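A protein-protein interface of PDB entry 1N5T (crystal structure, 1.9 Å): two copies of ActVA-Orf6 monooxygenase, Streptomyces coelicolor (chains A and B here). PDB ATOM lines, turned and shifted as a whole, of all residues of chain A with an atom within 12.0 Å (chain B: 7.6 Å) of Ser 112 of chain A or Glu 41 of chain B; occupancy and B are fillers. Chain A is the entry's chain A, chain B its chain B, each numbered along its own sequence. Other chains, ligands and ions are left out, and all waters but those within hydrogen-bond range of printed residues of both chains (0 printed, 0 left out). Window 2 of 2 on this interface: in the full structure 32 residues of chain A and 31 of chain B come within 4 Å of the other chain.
O of Leu 110 of chain A is in hydrogen-bond range of NE of Arg 40 of chain B (2.9 Å).
The backbone carbonyl oxygen (O) of Arg 40 of chain B sits at hydrogen-bond distance from the backbone NH (N) of Ser 112 of chain A, at 3.2 Å.
Of the 6 printed residues of chain A, 4 touch a printed residue of chain B.
Hydrophobic or aromatic side chains of chain A within 4 Å of the printed part of chain B: Ile 109 and Pro 111.
Hydrophobic or aromatic side chains of chain B that line the printed part of chain A: Phe 45.
No position is printed for both chains.
Of the 8 pairs that touch across the chains among the printed residues, none has its exchanged pair printed and touching as well.
Arg 40 of chain B touches Ile 109 of chain A.
Phe 45 of chain B touches Ile 109 of chain A (CZ to O, 3.3 Å).
Pro 111 of chain A touches Arg 40 of chain B (CA to O, 3.5 Å).
Pro 111 of chain A touches Phe 45 of chain B (CG to O, 3.8 Å).
Pro 111 of chain A touches Leu 46 of chain B (CD to O, 3.0 Å).
OXT of Ser 112 of chain A touches CG of Glu 41 of chain B (3.3 Å).
Of the printed residues of chain B, Ser 112 of chain A touches Arg 40 and Glu 41.
Glu 41 of chain B touches just one residue of chain A: Ser 112 (3.3 Å).
No residue of chain A comes within 4 Å of Glu 37 of chain B.
No residue of chain A comes within 4 Å of Val 42 of chain B.
Phe 45 of chain B touches just these residues of chain A: Ile 109 and Pro 111.
Printed residues of chain B within 4 Å of Leu 110 of chain A: Arg 40.
Of the printed residues of chain B, Pro 111 of chain A touches Arg 40, Phe 45 and Leu 46.
Gly 44 of chain B touches none of the printed residues of chain A.
Ala 108 of chain A touches none of the printed residues of chain B.
The nearest residue of chain B that does not touch Ser 112 of chain A is Glu 37 of chain B (5.2 Å).
The nearest residue of chain A that does not touch Glu 41 of chain B is Pro 111 of chain A (5.6 Å).
The side-chain carboxylate (OE2) of Glu 37 of chain B is in salt-bridge range of the guanidinium group (NH1) of Arg 40 of chain B.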
ATOM      1  N   ASN A   4      15.696   8.115   6.475  1.00  0.00           N
ATOM      2  CA  ASN A   4      15.219   8.670   5.221  1.00  0.00           C
ATOM      3  C   ASN A   4      15.081  10.181   5.282  1.00  0.00           C
ATOM      4  O   ASN A   4      14.574  10.772   4.321  1.00  0.00           O
ATOM      5  CB  ASN A   4      13.901   8.007   4.782  1.00  0.00           C
ATOM      6  CG  ASN A   4      12.757   8.285   5.730  1.00  0.00           C
ATOM      7  OD1 ASN A   4      12.949   8.388   6.940  1.00  0.00           O
ATOM      8  ND2 ASN A   4      11.547   8.395   5.162  1.00  0.00           N
ATOM      9  N   ALA A 108      13.973   4.706  -0.104  1.00  0.00           N
ATOM     10  CA  ALA A 108      13.798   4.074   1.202  1.00  0.00           C
ATOM     11  C   ALA A 108      12.378   3.572   1.357  1.00  0.00           C
ATOM     12  O   ALA A 108      11.433   4.107   0.725  1.00  0.00           O
ATOM     13  CB  ALA A 108      14.129   5.025   2.337  1.00  0.00           C
ATOM     14  N   ILE A 109      12.272   2.500   2.105  1.00  0.00           N
ATOM     15  CA  ILE A 109      10.931   1.943   2.389  1.00  0.00           C
ATOM     16  C   ILE A 109      10.686   2.025   3.884  1.00  0.00           C
ATOM     17  O   ILE A 109      11.510   1.424   4.626  1.00  0.00           O
ATOM     18  CB  ILE A 109      10.887   0.467   1.949  1.00  0.00           C
ATOM     19  CG1 ILE A 109      11.201   0.284   0.452  1.00  0.00           C
ATOM     20  CG2 ILE A 109       9.509  -0.093   2.284  1.00  0.00           C
ATOM     21  CD1 ILE A 109      11.242  -1.174   0.004  1.00  0.00           C
ATOM     22  N   LEU A 110       9.656   2.729   4.351  1.00  0.00           N
ATOM     23  CA  LEU A 110       9.385   2.781   5.803  1.00  0.00           C
ATOM     24  C   LEU A 110       8.041   2.143   6.099  1.00  0.00           C
ATOM     25  O   LEU A 110       7.253   1.937   5.171  1.00  0.00           O
ATOM     26  CB  LEU A 110       9.596   4.193   6.361  1.00  0.00           C
ATOM     27  CG  LEU A 110      11.088   4.391   6.782  1.00  0.00           C
ATOM     28  CD1 LEU A 110      11.855   4.971   5.619  1.00  0.00           C
ATOM     29  CD2 LEU A 110      11.300   5.170   8.050  1.00  0.00           C
ATOM     30  N   PRO A 111       7.789   1.621   7.298  1.00  0.00           N
ATOM     31  CA  PRO A 111       6.605   0.869   7.648  1.00  0.00           C
ATOM     32  C   PRO A 111       5.272   1.577   7.480  1.00  0.00           C
ATOM     33  O   PRO A 111       5.196   2.802   7.441  1.00  0.00           O
ATOM     34  CB  PRO A 111       6.771   0.422   9.094  1.00  0.00           C
ATOM     35  CG  PRO A 111       8.027   1.056   9.564  1.00  0.00           C
ATOM     36  CD  PRO A 111       8.678   1.817   8.461  1.00  0.00           C
ATOM     37  N   SER A 112       4.247   0.752   7.297  1.00  0.00           N
ATOM     38  CA  SER A 112       2.868   1.107   7.086  1.00  0.00           C
ATOM     39  C   SER A 112       2.107  -0.100   6.499  1.00  0.00           C
ATOM     40  O   SER A 112       1.939  -0.203   5.258  1.00  0.00           O
ATOM     41  CB  SER A 112       2.585   2.302   6.183  1.00  0.00           C
ATOM     42  OG  SER A 112       1.321   2.857   6.524  1.00  0.00           O
ATOM     43  OXT SER A 112       2.066  -1.054   7.332  1.00  0.00           O
ATOM     44  N   GLN B  36       6.603  -3.802  -4.126  1.00  0.00           N
ATOM     45  CA  GLN B  36       7.252  -4.240  -2.901  1.00  0.00           C
ATOM     46  C   GLN B  36       6.665  -3.582  -1.663  1.00  0.00           C
ATOM     47  O   GLN B  36       7.205  -3.730  -0.553  1.00  0.00           O
ATOM     48  CB  GLN B  36       8.756  -4.033  -2.957  1.00  0.00           C
ATOM     49  CG  GLN B  36       9.470  -4.446  -4.220  1.00  0.00           C
ATOM     50  CD  GLN B  36       9.082  -5.811  -4.757  1.00  0.00           C
ATOM     51  OE1 GLN B  36       9.104  -6.054  -5.972  1.00  0.00           O
ATOM     52  NE2 GLN B  36       8.710  -6.725  -3.863  1.00  0.00           N
ATOM     53  N   GLU B  37       5.472  -2.987  -1.736  1.00  0.00           N
ATOM     54  CA  GLU B  37       4.841  -2.419  -0.562  1.00  0.00           C
ATOM     55  C   GLU B  37       4.408  -3.476   0.453  1.00  0.00           C
ATOM     56  O   GLU B  37       4.302  -3.102   1.620  1.00  0.00           O
ATOM     57  CB  GLU B  37       3.698  -1.461  -0.902  1.00  0.00           C
ATOM     58  CG  GLU B  37       4.246  -0.107  -1.345  1.00  0.00           C
ATOM     59  CD  GLU B  37       3.621   1.067  -0.620  1.00  0.00           C
ATOM     60  OE1 GLU B  37       2.528   0.911  -0.024  1.00  0.00           O
ATOM     61  OE2 GLU B  37       4.234   2.169  -0.636  1.00  0.00           O
ATOM     62  N   TRP B  38       4.406  -4.783   0.151  1.00  0.00           N
ATOM     63  CA  TRP B  38       4.093  -5.760   1.200  1.00  0.00           C
ATOM     64  C   TRP B  38       5.124  -5.731   2.329  1.00  0.00           C
ATOM     65  O   TRP B  38       4.821  -5.932   3.524  1.00  0.00           O
ATOM     66  CB  TRP B  38       3.994  -7.169   0.601  1.00  0.00           C
ATOM     67  CG  TRP B  38       5.335  -7.627   0.086  1.00  0.00           C
ATOM     68  CD1 TRP B  38       5.916  -7.280  -1.106  1.00  0.00           C
ATOM     69  CD2 TRP B  38       6.253  -8.489   0.765  1.00  0.00           C
ATOM     70  NE1 TRP B  38       7.147  -7.906  -1.202  1.00  0.00           N
ATOM     71  CE2 TRP B  38       7.365  -8.652  -0.065  1.00  0.00           C
ATOM     72  CE3 TRP B  38       6.197  -9.177   1.988  1.00  0.00           C
ATOM     73  CZ2 TRP B  38       8.462  -9.448   0.291  1.00  0.00           C
ATOM     74  CZ3 TRP B  38       7.269  -9.970   2.353  1.00  0.00           C
ATOM     75  CH2 TRP B  38       8.390 -10.097   1.501  1.00  0.00           C
ATOM     76  N   ILE B  39       6.409  -5.426   1.988  1.00  0.00           N
ATOM     77  CA  ILE B  39       7.471  -5.341   3.019  1.00  0.00           C
ATOM     78  C   ILE B  39       7.166  -4.370   4.132  1.00  0.00           C
ATOM     79  O   ILE B  39       7.389  -4.621   5.346  1.00  0.00           O
ATOM     80  CB  ILE B  39       8.747  -4.834   2.276  1.00  0.00           C
ATOM     81  CG1 ILE B  39       9.150  -5.946   1.298  1.00  0.00           C
ATOM     82  CG2 ILE B  39       9.866  -4.599   3.262  1.00  0.00           C
ATOM     83  CD1 ILE B  39      10.233  -5.491   0.318  1.00  0.00           C
ATOM     84  N   ARG B  40       6.485  -3.274   3.802  1.00  0.00           N
ATOM     85  CA  ARG B  40       6.089  -2.268   4.765  1.00  0.00           C
ATOM     86  C   ARG B  40       5.213  -2.813   5.872  1.00  0.00           C
ATOM     87  O   ARG B  40       5.243  -2.257   6.980  1.00  0.00           O
ATOM     88  CB  ARG B  40       5.291  -1.131   4.055  1.00  0.00           C
ATOM     89  CG  ARG B  40       6.149  -0.512   2.954  1.00  0.00           C
ATOM     90  CD  ARG B  40       5.343   0.571   2.232  1.00  0.00           C
ATOM     91  NE  ARG B  40       5.268   1.755   3.063  1.00  0.00           N
ATOM     92  CZ  ARG B  40       4.422   2.769   3.063  1.00  0.00           C
ATOM     93  NH1 ARG B  40       3.424   2.872   2.180  1.00  0.00           N
ATOM     94  NH2 ARG B  40       4.598   3.714   3.989  1.00  0.00           N
ATOM     95  N   GLU B  41       4.440  -3.835   5.585  1.00  0.00           N
ATOM     96  CA  GLU B  41       3.558  -4.437   6.560  1.00  0.00           C
ATOM     97  C   GLU B  41       4.112  -5.677   7.198  1.00  0.00           C
ATOM     98  O   GLU B  41       3.371  -6.289   8.019  1.00  0.00           O
ATOM     99  CB  GLU B  41       2.224  -4.790   5.804  1.00  0.00           C
ATOM    100  CG  GLU B  41       1.657  -3.548   5.184  1.00  0.00           C
ATOM    101  CD  GLU B  41       0.335  -3.687   4.470  1.00  0.00           C
ATOM    102  OE1 GLU B  41      -0.241  -4.772   4.345  1.00  0.00           O
ATOM    103  OE2 GLU B  41      -0.159  -2.695   3.920  1.00  0.00           O
ATOM    104  N   VAL B  42       5.364  -6.075   6.880  1.00  0.00           N
ATOM    105  CA  VAL B  42       5.912  -7.265   7.558  1.00  0.00           C
ATOM    106  C   VAL B  42       6.132  -6.937   9.052  1.00  0.00           C
ATOM    107  O   VAL B  42       6.703  -5.888   9.346  1.00  0.00           O
ATOM    108  CB  VAL B  42       7.228  -7.740   6.943  1.00  0.00           C
ATOM    109  CG1 VAL B  42       7.908  -8.899   7.664  1.00  0.00           C
ATOM    110  CG2 VAL B  42       6.989  -8.166   5.471  1.00  0.00           C
ATOM    111  N   PRO B  43       5.741  -7.775   9.952  1.00  0.00           N
ATOM    112  CA  PRO B  43       5.869  -7.569  11.392  1.00  0.00           C
ATOM    113  C   PRO B  43       7.374  -7.494  11.742  1.00  0.00           C
ATOM    114  O   PRO B  43       8.104  -8.360  11.213  1.00  0.00           O
ATOM    115  CB  PRO B  43       5.271  -8.854  12.000  1.00  0.00           C
ATOM    116  CG  PRO B  43       4.368  -9.420  10.928  1.00  0.00           C
ATOM    117  CD  PRO B  43       4.978  -9.044   9.605  1.00  0.00           C
ATOM    118  N   GLY B  44       7.808  -6.477  12.443  1.00  0.00           N
ATOM    119  CA  GLY B  44       9.251  -6.360  12.852  1.00  0.00           C
ATOM    120  C   GLY B  44      10.045  -5.574  11.834  1.00  0.00           C
ATOM    121  O   GLY B  44      11.228  -5.215  12.154  1.00  0.00           O
ATOM    122  N   PHE B  45       9.509  -5.250  10.654  1.00  0.00           N
ATOM    123  CA  PHE B  45      10.259  -4.464   9.682  1.00  0.00           C
ATOM    124  C   PHE B  45      10.276  -3.013  10.132  1.00  0.00           C
ATOM    125  O   PHE B  45       9.215  -2.431  10.492  1.00  0.00           O
ATOM    126  CB  PHE B  45       9.649  -4.542   8.290  1.00  0.00           C
ATOM    127  CG  PHE B  45      10.179  -3.568   7.255  1.00  0.00           C
ATOM    128  CD1 PHE B  45      11.430  -3.739   6.669  1.00  0.00           C
ATOM    129  CD2 PHE B  45       9.411  -2.478   6.909  1.00  0.00           C
ATOM    130  CE1 PHE B  45      11.865  -2.845   5.702  1.00  0.00           C
ATOM    131  CE2 PHE B  45       9.865  -1.550   5.982  1.00  0.00           C
ATOM    132  CZ  PHE B  45      11.092  -1.749   5.347  1.00  0.00           C
ATOM    133  N   LEU B  46      11.481  -2.424  10.184  1.00  0.00           N
ATOM    134  CA  LEU B  46      11.547  -1.006  10.565  1.00  0.00           C
ATOM    135  C   LEU B  46      11.945  -0.098   9.404  1.00  0.00           C
ATOM    136  O   LEU B  46      11.392   1.023   9.320  1.00  0.00           O
ATOM    137  CB  LEU B  46      12.461  -0.790  11.771  1.00  0.00           C
ATOM    138  CG  LEU B  46      11.950  -1.525  13.041  1.00  0.00           C
ATOM    139  CD1 LEU B  46      13.087  -1.558  14.043  1.00  0.00           C
ATOM    140  CD2 LEU B  46      10.701  -0.852  13.605  1.00  0.00           C
ATOM    141  N   ARG B  80       7.202 -14.128  -1.111  1.00  0.00           N
ATOM    142  CA  ARG B  80       7.474 -12.882  -1.790  1.00  0.00           C
ATOM    143  C   ARG B  80       8.944 -12.446  -1.706  1.00  0.00           C
ATOM    144  O   ARG B  80       9.378 -11.657  -2.533  1.00  0.00           O
ATOM    145  CB  ARG B  80       6.544 -11.757  -1.339  1.00  0.00           C
ATOM    146  CG  ARG B  80       5.107 -12.034  -1.826  1.00  0.00           C
ATOM    147  CD  ARG B  80       4.140 -11.082  -1.102  1.00  0.00           C
ATOM    148  NE  ARG B  80       3.890 -11.478   0.304  1.00  0.00           N
ATOM    149  CZ  ARG B  80       2.945 -10.935   1.078  1.00  0.00           C
ATOM    150  NH1 ARG B  80       2.128  -9.992   0.595  1.00  0.00           N
ATOM    151  NH2 ARG B  80       2.759 -11.309   2.336  1.00  0.00           N
